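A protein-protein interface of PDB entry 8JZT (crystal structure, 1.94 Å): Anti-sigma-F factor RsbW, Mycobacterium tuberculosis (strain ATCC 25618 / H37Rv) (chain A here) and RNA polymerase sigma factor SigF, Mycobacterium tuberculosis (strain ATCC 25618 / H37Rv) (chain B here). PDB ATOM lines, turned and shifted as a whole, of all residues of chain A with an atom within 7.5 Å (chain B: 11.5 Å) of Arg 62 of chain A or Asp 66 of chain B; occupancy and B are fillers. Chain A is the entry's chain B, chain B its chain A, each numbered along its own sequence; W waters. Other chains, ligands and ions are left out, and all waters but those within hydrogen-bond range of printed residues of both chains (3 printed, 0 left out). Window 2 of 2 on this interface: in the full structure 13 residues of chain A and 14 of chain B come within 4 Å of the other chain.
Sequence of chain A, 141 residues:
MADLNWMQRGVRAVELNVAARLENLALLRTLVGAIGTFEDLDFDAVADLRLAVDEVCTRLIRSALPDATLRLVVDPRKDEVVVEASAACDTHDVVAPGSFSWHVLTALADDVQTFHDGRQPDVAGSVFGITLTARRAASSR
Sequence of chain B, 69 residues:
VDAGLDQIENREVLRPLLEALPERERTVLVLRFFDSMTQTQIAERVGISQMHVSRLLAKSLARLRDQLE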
ATOM      1  N   ALA A  20     -25.543  21.232 -29.891  1.00  0.00           N
ATOM      2  CA  ALA A  20     -25.966  20.184 -28.950  1.00  0.00           C
ATOM      3  C   ALA A  20     -27.141  19.416 -29.556  1.00  0.00           C
ATOM      4  O   ALA A  20     -28.292  19.544 -29.135  1.00  0.00           O
ATOM      5  CB  ALA A  20     -26.334  20.806 -27.604  1.00  0.00           C
ATOM      6  N   ARG A  21     -26.821  18.613 -30.583  1.00  0.00           N
ATOM      7  CA  ARG A  21     -27.792  17.859 -31.369  1.00  0.00           C
ATOM      8  C   ARG A  21     -27.388  16.401 -31.450  1.00  0.00           C
ATOM      9  O   ARG A  21     -26.205  16.089 -31.602  1.00  0.00           O
ATOM     10  CB  ARG A  21     -27.924  18.422 -32.795  1.00  0.00           C
ATOM     11  CG  ARG A  21     -28.618  19.770 -32.824  1.00  0.00           C
ATOM     12  CD  ARG A  21     -30.128  19.580 -32.949  1.00  0.00           C
ATOM     13  NE  ARG A  21     -30.501  18.871 -34.170  1.00  0.00           N
ATOM     14  CZ  ARG A  21     -30.800  19.492 -35.305  1.00  0.00           C
ATOM     15  NH1 ARG A  21     -30.774  20.814 -35.394  1.00  0.00           N
ATOM     16  NH2 ARG A  21     -31.145  18.773 -36.372  1.00  0.00           N
ATOM     17  N   LEU A  22     -28.375  15.498 -31.376  1.00  0.00           N
ATOM     18  CA  LEU A  22     -28.031  14.070 -31.386  1.00  0.00           C
ATOM     19  C   LEU A  22     -27.265  13.675 -32.650  1.00  0.00           C
ATOM     20  O   LEU A  22     -26.466  12.731 -32.615  1.00  0.00           O
ATOM     21  CB  LEU A  22     -29.271  13.169 -31.251  1.00  0.00           C
ATOM     22  CG  LEU A  22     -30.298  13.184 -32.370  1.00  0.00           C
ATOM     23  CD1 LEU A  22     -29.951  12.121 -33.399  1.00  0.00           C
ATOM     24  CD2 LEU A  22     -31.671  12.833 -31.781  1.00  0.00           C
ATOM     25  N   LEU A  25     -23.351  13.448 -32.113  1.00  0.00           N
ATOM     26  CA  LEU A  25     -22.720  12.567 -31.142  1.00  0.00           C
ATOM     27  C   LEU A  25     -21.667  11.683 -31.815  1.00  0.00           C
ATOM     28  O   LEU A  25     -20.604  11.426 -31.241  1.00  0.00           O
ATOM     29  CB  LEU A  25     -23.791  11.727 -30.434  1.00  0.00           C
ATOM     30  CG  LEU A  25     -24.602  12.479 -29.360  1.00  0.00           C
ATOM     31  CD1 LEU A  25     -25.932  11.721 -28.988  1.00  0.00           C
ATOM     32  CD2 LEU A  25     -23.734  12.775 -28.123  1.00  0.00           C
ATOM     33  N   VAL A  56     -21.575  11.199 -21.000  1.00  0.00           N
ATOM     34  CA  VAL A  56     -21.760  12.613 -20.680  1.00  0.00           C
ATOM     35  C   VAL A  56     -22.359  13.365 -21.865  1.00  0.00           C
ATOM     36  O   VAL A  56     -23.343  14.104 -21.732  1.00  0.00           O
ATOM     37  CB  VAL A  56     -20.412  13.213 -20.248  1.00  0.00           C
ATOM     38  CG1 VAL A  56     -20.473  14.733 -20.258  1.00  0.00           C
ATOM     39  CG2 VAL A  56     -20.007  12.648 -18.832  1.00  0.00           C
ATOM     40  N   CYS A  57     -21.756  13.213 -23.044  1.00  0.00           N
ATOM     41  CA  CYS A  57     -22.224  13.988 -24.187  1.00  0.00           C
ATOM     42  C   CYS A  57     -23.637  13.602 -24.574  1.00  0.00           C
ATOM     43  O   CYS A  57     -24.434  14.468 -24.947  1.00  0.00           O
ATOM     44  CB  CYS A  57     -21.300  13.787 -25.377  1.00  0.00           C
ATOM     45  SG  CYS A  57     -19.704  14.596 -25.189  1.00  0.00           S
ATOM     46  N   THR A  58     -23.957  12.300 -24.521  1.00  0.00           N
ATOM     47  CA  THR A  58     -25.303  11.850 -24.865  1.00  0.00           C
ATOM     48  C   THR A  58     -26.352  12.406 -23.898  1.00  0.00           C
ATOM     49  O   THR A  58     -27.431  12.840 -24.321  1.00  0.00           O
ATOM     50  CB  THR A  58     -25.332  10.319 -24.889  1.00  0.00           C
ATOM     51  OG1 THR A  58     -24.420   9.858 -25.892  1.00  0.00           O
ATOM     52  CG2 THR A  58     -26.715   9.806 -25.248  1.00  0.00           C
ATOM     53  N   ARG A  59     -26.062  12.394 -22.598  1.00  0.00           N
ATOM     54  CA  ARG A  59     -27.034  12.883 -21.631  1.00  0.00           C
ATOM     55  C   ARG A  59     -27.195  14.394 -21.730  1.00  0.00           C
ATOM     56  O   ARG A  59     -28.312  14.907 -21.614  1.00  0.00           O
ATOM     57  CB  ARG A  59     -26.617  12.484 -20.209  1.00  0.00           C
ATOM     58  CG  ARG A  59     -26.693  10.987 -19.906  1.00  0.00           C
ATOM     59  CD  ARG A  59     -28.118  10.512 -19.595  1.00  0.00           C
ATOM     60  NE  ARG A  59     -28.120   9.151 -19.053  1.00  0.00           N
ATOM     61  CZ  ARG A  59     -29.165   8.330 -19.016  1.00  0.00           C
ATOM     62  NH1 ARG A  59     -30.351   8.686 -19.490  1.00  0.00           N
ATOM     63  NH2 ARG A  59     -29.025   7.126 -18.460  1.00  0.00           N
ATOM     64  N   LEU A  60     -26.092  15.124 -21.948  1.00  0.00           N
ATOM     65  CA  LEU A  60     -26.201  16.570 -22.117  1.00  0.00           C
ATOM     66  C   LEU A  60     -27.026  16.902 -23.354  1.00  0.00           C
ATOM     67  O   LEU A  60     -27.939  17.733 -23.307  1.00  0.00           O
ATOM     68  CB  LEU A  60     -24.807  17.179 -22.221  1.00  0.00           C
ATOM     69  CG  LEU A  60     -24.078  17.245 -20.878  1.00  0.00           C
ATOM     70  CD1 LEU A  60     -22.607  17.574 -21.160  1.00  0.00           C
ATOM     71  CD2 LEU A  60     -24.729  18.267 -19.906  1.00  0.00           C
ATOM     72  N   ILE A  61     -26.723  16.250 -24.476  1.00  0.00           N
ATOM     73  CA  ILE A  61     -27.397  16.615 -25.720  1.00  0.00           C
ATOM     74  C   ILE A  61     -28.868  16.194 -25.674  1.00  0.00           C
ATOM     75  O   ILE A  61     -29.752  16.919 -26.147  1.00  0.00           O
ATOM     76  CB  ILE A  61     -26.635  16.010 -26.920  1.00  0.00           C
ATOM     77  CG1 ILE A  61     -25.366  16.826 -27.187  1.00  0.00           C
ATOM     78  CG2 ILE A  61     -27.512  15.972 -28.140  1.00  0.00           C
ATOM     79  CD1 ILE A  61     -24.523  16.331 -28.371  1.00  0.00           C
ATOM     80  N   ARG A  62     -29.170  15.048 -25.064  1.00  0.00           N
ATOM     81  CA  ARG A  62     -30.578  14.687 -24.878  1.00  0.00           C
ATOM     82  C   ARG A  62     -31.350  15.712 -24.054  1.00  0.00           C
ATOM     83  O   ARG A  62     -32.558  15.878 -24.262  1.00  0.00           O
ATOM     84  CB  ARG A  62     -30.687  13.325 -24.223  1.00  0.00           C
ATOM     85  CG  ARG A  62     -30.356  12.243 -25.191  1.00  0.00           C
ATOM     86  CD  ARG A  62     -30.711  10.931 -24.606  1.00  0.00           C
ATOM     87  NE  ARG A  62     -30.431   9.852 -25.537  1.00  0.00           N
ATOM     88  CZ  ARG A  62     -30.707   8.591 -25.263  1.00  0.00           C
ATOM     89  NH1 ARG A  62     -31.195   8.239 -24.082  1.00  0.00           N
ATOM     90  NH2 ARG A  62     -30.480   7.665 -26.185  1.00  0.00           N
ATOM     91  N   SER A  63     -30.689  16.406 -23.126  1.00  0.00           N
ATOM     92  CA  SER A  63     -31.366  17.387 -22.273  1.00  0.00           C
ATOM     93  C   SER A  63     -31.190  18.815 -22.757  1.00  0.00           C
ATOM     94  O   SER A  63     -31.733  19.732 -22.132  1.00  0.00           O
ATOM     95  CB  SER A  63     -30.857  17.289 -20.821  1.00  0.00           C
ATOM     96  OG  SER A  63     -31.384  16.134 -20.172  1.00  0.00           O
ATOM     97  N   ALA A  64     -30.460  19.018 -23.851  1.00  0.00           N
ATOM     98  CA  ALA A  64     -30.086  20.348 -24.292  1.00  0.00           C
ATOM     99  C   ALA A  64     -31.309  21.169 -24.695  1.00  0.00           C
ATOM    100  O   ALA A  64     -32.286  20.661 -25.259  1.00  0.00           O
ATOM    101  CB  ALA A  64     -29.117  20.267 -25.472  1.00  0.00           C
ATOM    102  N   LEU A  65     -31.236  22.466 -24.413  1.00  0.00           N
ATOM    103  CA  LEU A  65     -32.267  23.379 -24.883  1.00  0.00           C
ATOM    104  C   LEU A  65     -32.113  23.555 -26.393  1.00  0.00           C
ATOM    105  O   LEU A  65     -31.057  23.240 -26.954  1.00  0.00           O
ATOM    106  CB  LEU A  65     -32.130  24.714 -24.158  1.00  0.00           C
ATOM    107  CG  LEU A  65     -32.428  24.689 -22.648  1.00  0.00           C
ATOM    108  CD1 LEU A  65     -32.123  26.045 -21.989  1.00  0.00           C
ATOM    109  CD2 LEU A  65     -33.899  24.317 -22.428  1.00  0.00           C
ATOM    110  N   CYS A  89     -29.158  23.231 -20.665  1.00  0.00           N
ATOM    111  CA  CYS A  89     -30.030  22.070 -20.532  1.00  0.00           C
ATOM    112  C   CYS A  89     -31.374  22.452 -19.913  1.00  0.00           C
ATOM    113  O   CYS A  89     -31.518  23.514 -19.307  1.00  0.00           O
ATOM    114  CB  CYS A  89     -29.358  20.995 -19.674  1.00  0.00           C
ATOM    115  SG  CYS A  89     -27.962  20.267 -20.536  1.00  0.00           S
ATOM    116  N   ASP A  90     -32.354  21.559 -20.059  1.00  0.00           N
ATOM    117  CA  ASP A  90     -33.723  21.793 -19.604  1.00  0.00           C
ATOM    118  C   ASP A  90     -33.982  21.301 -18.189  1.00  0.00           C
ATOM    119  O   ASP A  90     -35.143  21.245 -17.764  1.00  0.00           O
ATOM    120  CB  ASP A  90     -34.727  21.153 -20.565  1.00  0.00           C
ATOM    121  CG  ASP A  90     -34.613  19.633 -20.638  1.00  0.00           C
ATOM    122  OD1 ASP A  90     -33.902  18.989 -19.846  1.00  0.00           O
ATOM    123  OD2 ASP A  90     -35.252  19.067 -21.531  1.00  0.00           O
ATOM    124  N   VAL A  94     -28.455  16.785 -14.848  1.00  0.00           N
ATOM    125  CA  VAL A  94     -28.572  15.825 -15.934  1.00  0.00           C
ATOM    126  C   VAL A  94     -28.176  14.412 -15.498  1.00  0.00           C
ATOM    127  O   VAL A  94     -28.552  13.433 -16.155  1.00  0.00           O
ATOM    128  CB  VAL A  94     -27.730  16.376 -17.106  1.00  0.00           C
ATOM    129  CG1 VAL A  94     -27.360  15.321 -18.063  1.00  0.00           C
ATOM    130  CG2 VAL A  94     -28.479  17.525 -17.804  1.00  0.00           C
ATOM    131  N   PHE A 100     -28.435   5.498 -12.585  1.00  0.00           N
ATOM    132  CA  PHE A 100     -27.556   4.561 -13.264  1.00  0.00           C
ATOM    133  C   PHE A 100     -26.428   5.298 -13.978  1.00  0.00           C
ATOM    134  O   PHE A 100     -25.265   4.903 -13.884  1.00  0.00           O
ATOM    135  CB  PHE A 100     -28.357   3.714 -14.251  1.00  0.00           C
ATOM    136  CG  PHE A 100     -27.520   2.733 -15.019  1.00  0.00           C
ATOM    137  CD1 PHE A 100     -27.006   1.617 -14.387  1.00  0.00           C
ATOM    138  CD2 PHE A 100     -27.259   2.922 -16.373  1.00  0.00           C
ATOM    139  CE1 PHE A 100     -26.233   0.694 -15.093  1.00  0.00           C
ATOM    140  CE2 PHE A 100     -26.488   2.005 -17.091  1.00  0.00           C
ATOM    141  CZ  PHE A 100     -25.975   0.892 -16.452  1.00  0.00           C
ATOM    142  N   VAL B  13     -33.087  -4.168  -9.859  1.00  0.00           N
ATOM    143  CA  VAL B  13     -33.741  -3.609 -11.039  1.00  0.00           C
ATOM    144  C   VAL B  13     -32.954  -3.953 -12.296  1.00  0.00           C
ATOM    145  O   VAL B  13     -33.533  -4.207 -13.359  1.00  0.00           O
ATOM    146  CB  VAL B  13     -33.917  -2.086 -10.882  1.00  0.00           C
ATOM    147  CG1 VAL B  13     -34.787  -1.528 -12.002  1.00  0.00           C
ATOM    148  CG2 VAL B  13     -34.515  -1.760  -9.520  1.00  0.00           C
ATOM    149  N   LEU B  14     -31.625  -3.975 -12.195  1.00  0.00           N
ATOM    150  CA  LEU B  14     -30.807  -4.224 -13.375  1.00  0.00           C
ATOM    151  C   LEU B  14     -30.892  -5.673 -13.832  1.00  0.00           C
ATOM    152  O   LEU B  14     -30.748  -5.945 -15.031  1.00  0.00           O
ATOM    153  CB  LEU B  14     -29.352  -3.843 -13.099  1.00  0.00           C
ATOM    154  CG  LEU B  14     -28.937  -2.445 -13.556  1.00  0.00           C
ATOM    155  CD1 LEU B  14     -29.723  -1.365 -12.824  1.00  0.00           C
ATOM    156  CD2 LEU B  14     -27.445  -2.246 -13.364  1.00  0.00           C
ATOM    157  N   LEU B  17     -33.021  -6.573 -16.780  1.00  0.00           N
ATOM    158  CA  LEU B  17     -32.486  -5.889 -17.950  1.00  0.00           C
ATOM    159  C   LEU B  17     -31.193  -6.547 -18.419  1.00  0.00           C
ATOM    160  O   LEU B  17     -30.926  -6.620 -19.624  1.00  0.00           O
ATOM    161  CB  LEU B  17     -32.259  -4.414 -17.625  1.00  0.00           C
ATOM    162  CG  LEU B  17     -33.519  -3.643 -17.207  1.00  0.00           C
ATOM    163  CD1 LEU B  17     -33.150  -2.264 -16.655  1.00  0.00           C
ATOM    164  CD2 LEU B  17     -34.567  -3.556 -18.318  1.00  0.00           C
ATOM    165  N   ALA B  20     -31.901  -9.635 -20.299  1.00  0.00           N
ATOM    166  CA  ALA B  20     -32.366  -9.305 -21.639  1.00  0.00           C
ATOM    167  C   ALA B  20     -31.220  -8.971 -22.586  1.00  0.00           C
ATOM    168  O   ALA B  20     -31.419  -8.987 -23.806  1.00  0.00           O
ATOM    169  CB  ALA B  20     -33.356  -8.138 -21.585  1.00  0.00           C
ATOM    170  N   LEU B  21     -30.040  -8.658 -22.053  1.00  0.00           N
ATOM    171  CA  LEU B  21     -28.896  -8.353 -22.893  1.00  0.00           C
ATOM    172  C   LEU B  21     -28.471  -9.599 -23.665  1.00  0.00           C
ATOM    173  O   LEU B  21     -28.662 -10.724 -23.193  1.00  0.00           O
ATOM    174  CB  LEU B  21     -27.722  -7.854 -22.047  1.00  0.00           C
ATOM    175  CG  LEU B  21     -27.874  -6.488 -21.378  1.00  0.00           C
ATOM    176  CD1 LEU B  21     -26.559  -6.010 -20.778  1.00  0.00           C
ATOM    177  CD2 LEU B  21     -28.411  -5.484 -22.379  1.00  0.00           C
ATOM    178  N   GLU B  25     -22.742  -9.560 -24.347  1.00  0.00           N
ATOM    179  CA  GLU B  25     -22.865  -8.218 -23.788  1.00  0.00           C
ATOM    180  C   GLU B  25     -22.967  -8.272 -22.268  1.00  0.00           C
ATOM    181  O   GLU B  25     -22.318  -7.489 -21.563  1.00  0.00           O
ATOM    182  CB  GLU B  25     -24.093  -7.518 -24.377  1.00  0.00           C
ATOM    183  CG  GLU B  25     -23.855  -6.957 -25.770  1.00  0.00           C
ATOM    184  CD  GLU B  25     -25.030  -6.140 -26.276  1.00  0.00           C
ATOM    185  OE1 GLU B  25     -25.611  -5.374 -25.468  1.00  0.00           O
ATOM    186  OE2 GLU B  25     -25.380  -6.277 -27.470  1.00  0.00           O
ATOM    187  N   LEU B  29     -20.359  -6.634 -19.562  1.00  0.00           N
ATOM    188  CA  LEU B  29     -20.839  -5.589 -18.658  1.00  0.00           C
ATOM    189  C   LEU B  29     -20.594  -5.946 -17.195  1.00  0.00           C
ATOM    190  O   LEU B  29     -20.150  -5.100 -16.405  1.00  0.00           O
ATOM    191  CB  LEU B  29     -22.322  -5.334 -18.883  1.00  0.00           C
ATOM    192  CG  LEU B  29     -22.767  -3.965 -18.370  1.00  0.00           C
ATOM    193  CD1 LEU B  29     -22.364  -2.854 -19.313  1.00  0.00           C
ATOM    194  CD2 LEU B  29     -24.252  -3.966 -18.131  1.00  0.00           C
ATOM    195  N   LEU B  57     -19.290  -2.959 -24.606  1.00  0.00           N
ATOM    196  CA  LEU B  57     -19.630  -2.086 -23.486  1.00  0.00           C
ATOM    197  C   LEU B  57     -20.460  -0.899 -23.963  1.00  0.00           C
ATOM    198  O   LEU B  57     -21.492  -0.567 -23.364  1.00  0.00           O
ATOM    199  CB  LEU B  57     -18.359  -1.601 -22.788  1.00  0.00           C
ATOM    200  CG  LEU B  57     -17.704  -2.656 -21.881  1.00  0.00           C
ATOM    201  CD1 LEU B  57     -16.356  -2.148 -21.375  1.00  0.00           C
ATOM    202  CD2 LEU B  57     -18.648  -3.085 -20.713  1.00  0.00           C
ATOM    203  N   ALA B  58     -20.024  -0.251 -25.051  1.00  0.00           N
ATOM    204  CA  ALA B  58     -20.743   0.917 -25.563  1.00  0.00           C
ATOM    205  C   ALA B  58     -22.174   0.546 -25.929  1.00  0.00           C
ATOM    206  O   ALA B  58     -23.139   1.210 -25.514  1.00  0.00           O
ATOM    207  CB  ALA B  58     -19.997   1.494 -26.768  1.00  0.00           C
ATOM    208  N   LYS B  59     -22.324  -0.542 -26.686  1.00  0.00           N
ATOM    209  CA  LYS B  59     -23.642  -1.034 -27.069  1.00  0.00           C
ATOM    210  C   LYS B  59     -24.529  -1.272 -25.847  1.00  0.00           C
ATOM    211  O   LYS B  59     -25.653  -0.760 -25.778  1.00  0.00           O
ATOM    212  CB  LYS B  59     -23.468  -2.317 -27.872  1.00  0.00           C
ATOM    213  CG  LYS B  59     -24.591  -2.623 -28.783  1.00  0.00           C
ATOM    214  CD  LYS B  59     -24.091  -3.033 -30.150  1.00  0.00           C
ATOM    215  CE  LYS B  59     -23.905  -4.521 -30.229  1.00  0.00           C
ATOM    216  NZ  LYS B  59     -22.946  -4.883 -31.317  1.00  0.00           N
ATOM    217  N   SER B  60     -24.029  -2.037 -24.860  1.00  0.00           N
ATOM    218  CA  SER B  60     -24.854  -2.403 -23.706  1.00  0.00           C
ATOM    219  C   SER B  60     -25.215  -1.194 -22.858  1.00  0.00           C
ATOM    220  O   SER B  60     -26.330  -1.115 -22.321  1.00  0.00           O
ATOM    221  CB  SER B  60     -24.147  -3.438 -22.830  1.00  0.00           C
ATOM    222  OG  SER B  60     -23.645  -4.505 -23.597  1.00  0.00           O
ATOM    223  N   LEU B  61     -24.275  -0.267 -22.683  1.00  0.00           N
ATOM    224  CA  LEU B  61     -24.595   0.945 -21.946  1.00  0.00           C
ATOM    225  C   LEU B  61     -25.653   1.754 -22.680  1.00  0.00           C
ATOM    226  O   LEU B  61     -26.515   2.363 -22.045  1.00  0.00           O
ATOM    227  CB  LEU B  61     -23.335   1.778 -21.715  1.00  0.00           C
ATOM    228  CG  LEU B  61     -22.351   1.091 -20.756  1.00  0.00           C
ATOM    229  CD1 LEU B  61     -21.014   1.841 -20.719  1.00  0.00           C
ATOM    230  CD2 LEU B  61     -22.960   0.983 -19.366  1.00  0.00           C
ATOM    231  N   ALA B  62     -25.606   1.761 -24.019  1.00  0.00           N
ATOM    232  CA  ALA B  62     -26.619   2.484 -24.788  1.00  0.00           C
ATOM    233  C   ALA B  62     -28.004   1.865 -24.613  1.00  0.00           C
ATOM    234  O   ALA B  62     -29.005   2.589 -24.546  1.00  0.00           O
ATOM    235  CB  ALA B  62     -26.232   2.523 -26.263  1.00  0.00           C
ATOM    236  N   ARG B  63     -28.089   0.530 -24.560  1.00  0.00           N
ATOM    237  CA  ARG B  63     -29.374  -0.121 -24.297  1.00  0.00           C
ATOM    238  C   ARG B  63     -29.871   0.195 -22.892  1.00  0.00           C
ATOM    239  O   ARG B  63     -31.031   0.582 -22.703  1.00  0.00           O
ATOM    240  CB  ARG B  63     -29.268  -1.640 -24.458  1.00  0.00           C
ATOM    241  CG  ARG B  63     -28.701  -2.144 -25.762  1.00  0.00           C
ATOM    242  CD  ARG B  63     -28.683  -3.670 -25.735  1.00  0.00           C
ATOM    243  NE  ARG B  63     -27.813  -4.241 -26.755  1.00  0.00           N
ATOM    244  CZ  ARG B  63     -28.212  -4.505 -27.988  1.00  0.00           C
ATOM    245  NH1 ARG B  63     -29.444  -4.226 -28.385  1.00  0.00           N
ATOM    246  NH2 ARG B  63     -27.347  -5.037 -28.853  1.00  0.00           N
ATOM    247  N   LEU B  64     -29.014  -0.007 -21.887  1.00  0.00           N
ATOM    248  CA  LEU B  64     -29.414   0.221 -20.504  1.00  0.00           C
ATOM    249  C   LEU B  64     -29.745   1.678 -20.255  1.00  0.00           C
ATOM    250  O   LEU B  64     -30.573   1.987 -19.391  1.00  0.00           O
ATOM    251  CB  LEU B  64     -28.297  -0.221 -19.565  1.00  0.00           C
ATOM    252  CG  LEU B  64     -28.104  -1.719 -19.427  1.00  0.00           C
ATOM    253  CD1 LEU B  64     -27.047  -1.955 -18.381  1.00  0.00           C
ATOM    254  CD2 LEU B  64     -29.401  -2.346 -18.994  1.00  0.00           C
ATOM    255  N   ARG B  65     -29.111   2.582 -21.002  1.00  0.00           N
ATOM    256  CA  ARG B  65     -29.337   4.012 -20.821  1.00  0.00           C
ATOM    257  C   ARG B  65     -30.806   4.377 -20.975  1.00  0.00           C
ATOM    258  O   ARG B  65     -31.298   5.283 -20.294  1.00  0.00           O
ATOM    259  CB  ARG B  65     -28.497   4.796 -21.832  1.00  0.00           C
ATOM    260  CG  ARG B  65     -28.438   6.288 -21.612  1.00  0.00           C
ATOM    261  CD  ARG B  65     -27.110   6.824 -22.161  1.00  0.00           C
ATOM    262  NE  ARG B  65     -26.912   6.372 -23.531  1.00  0.00           N
ATOM    263  CZ  ARG B  65     -25.737   6.216 -24.126  1.00  0.00           C
ATOM    264  NH1 ARG B  65     -24.597   6.370 -23.468  1.00  0.00           N
ATOM    265  NH2 ARG B  65     -25.704   5.883 -25.414  1.00  0.00           N
ATOM    266  N   ASP B  66     -31.517   3.686 -21.857  1.00  0.00           N
ATOM    267  CA  ASP B  66     -32.875   4.049 -22.231  1.00  0.00           C
ATOM    268  C   ASP B  66     -33.921   3.243 -21.485  1.00  0.00           C
ATOM    269  O   ASP B  66     -35.109   3.522 -21.613  1.00  0.00           O
ATOM    270  CB  ASP B  66     -33.051   3.880 -23.742  1.00  0.00           C
ATOM    271  CG  ASP B  66     -32.094   4.763 -24.527  1.00  0.00           C
ATOM    272  OD1 ASP B  66     -31.401   5.573 -23.874  1.00  0.00           O
ATOM    273  OD2 ASP B  66     -32.016   4.638 -25.771  1.00  0.00           O
ATOM    274  N   GLN B  67     -33.503   2.248 -20.718  1.00  0.00           N
ATOM    275  CA  GLN B  67     -34.399   1.447 -19.904  1.00  0.00           C
ATOM    276  C   GLN B  67     -34.365   1.868 -18.440  1.00  0.00           C
ATOM    277  O   GLN B  67     -35.033   1.247 -17.611  1.00  0.00           O
ATOM    278  CB  GLN B  67     -34.018  -0.027 -20.051  1.00  0.00           C
ATOM    279  CG  GLN B  67     -34.179  -0.560 -21.481  1.00  0.00           C
ATOM    280  CD  GLN B  67     -33.452  -1.878 -21.697  1.00  0.00           C
ATOM    281  OE1 GLN B  67     -32.646  -2.295 -20.869  1.00  0.00           O
ATOM    282  NE2 GLN B  67     -33.704  -2.517 -22.828  1.00  0.00           N
ATOM    283  N   LEU B  68     -33.621   2.919 -18.110  1.00  0.00           N
ATOM    284  CA  LEU B  68     -33.290   3.208 -16.726  1.00  0.00           C
ATOM    285  C   LEU B  68     -33.292   4.707 -16.455  1.00  0.00           C
ATOM    286  O   LEU B  68     -32.287   5.387 -16.690  1.00  0.00           O
ATOM    287  CB  LEU B  68     -31.916   2.625 -16.396  1.00  0.00           C
ATOM    288  CG  LEU B  68     -31.843   1.228 -15.789  1.00  0.00           C
ATOM    289  CD1 LEU B  68     -30.444   0.686 -15.958  1.00  0.00           C
ATOM    290  CD2 LEU B  68     -32.251   1.225 -14.327  1.00  0.00           C
HETATM  291  O   HOH W   1     -25.262   8.237 -27.785  1.00  0.00           O
HETATM  292  O   HOH W   2     -29.159   4.857 -25.591  1.00  0.00           O
HETATM  293  O   HOH W   3     -31.250   5.824 -13.406  1.00  0.00           O
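Of chain B, only Arg 65 (3.8 Å) comes within 4 Å of Thr 58 of chain A. Of chain B, only Arg 65 comes within 4 Å of Arg 59 of chain A. Arg 62 of chain A touches just one residue of chain B: Asp 66 (2.7 Å). No residue of chain B comes within 4 Å of Ser 63 of chain A. No residue of chain B comes within 4 Å of Ala 64 of chain A. Of the printed residues of chain A, Leu 14 of chain B touches Phe 100 (3.6 Å). Ala 20 of chain B touches none of the printed residues of chain A. Of the printed residues of chain A, Leu 64 of chain B touches Phe 100 (3.6 Å).
Water W2 lies within hydrogen-bond range of the backbone carbonyl oxygen (O) of Ala 62 of chain B (2.5 Å), the side-chain carboxylate (OD2) of Asp 66 of chain B (2.9 Å), the guanidinium group (NH2) of Arg 62 of chain A (3.2 Å) and the guanidinium group (NE) of Arg 65 of chain B (3.4 Å). Water W1 bridges the side-chain hydroxyl (OG1) of Thr 58 of chain A (2.6 Å) and the guanidinium group (NH2) of Arg 65 of chain B (3.4 Å). Water W3 lies within hydrogen-bond range of the backbone NH (N) of Phe 100 of chain A and the backbone carbonyl oxygen (O) of Leu 68 of chain B.
CG2 of Thr 58 of chain A touches NE of Arg 65 of chain B (3.8 Å). CD2 of Leu 14 of chain B touches CE1 of Phe 100 of chain A, at 3.6 Å. Leu 64 of chain B touches Phe 100 of chain A (CD1 to CZ, 3.6 Å). Phe 100 of chain A touches Leu 68 of chain B.
NH1 of Arg 62 of chain A is in salt-bridge range of OD1 of Asp 66 of chain B (2.7 Å). NH2 of Arg 59 of chain A lies close to O of Arg 65 of chain B, at 3.5 Å.
Of the 18 printed residues of chain A, 4 touch a printed residue of chain B. Printed residues of chain A that touch a printed residue of chain B: Thr 58, Arg 59, Arg 62 and Phe 100. Along chain A the printed residues that touch a printed residue of chain B span positions 58 to 100. Among the printed residues, 6 pairs touch across the chains. Among the printed residues, Asp or Glu carboxylates within 4 Å of a Lys or Arg side-chain nitrogen of the other chain: Arg 62 of chain A with Asp 66 of chain B (2.7 Å).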
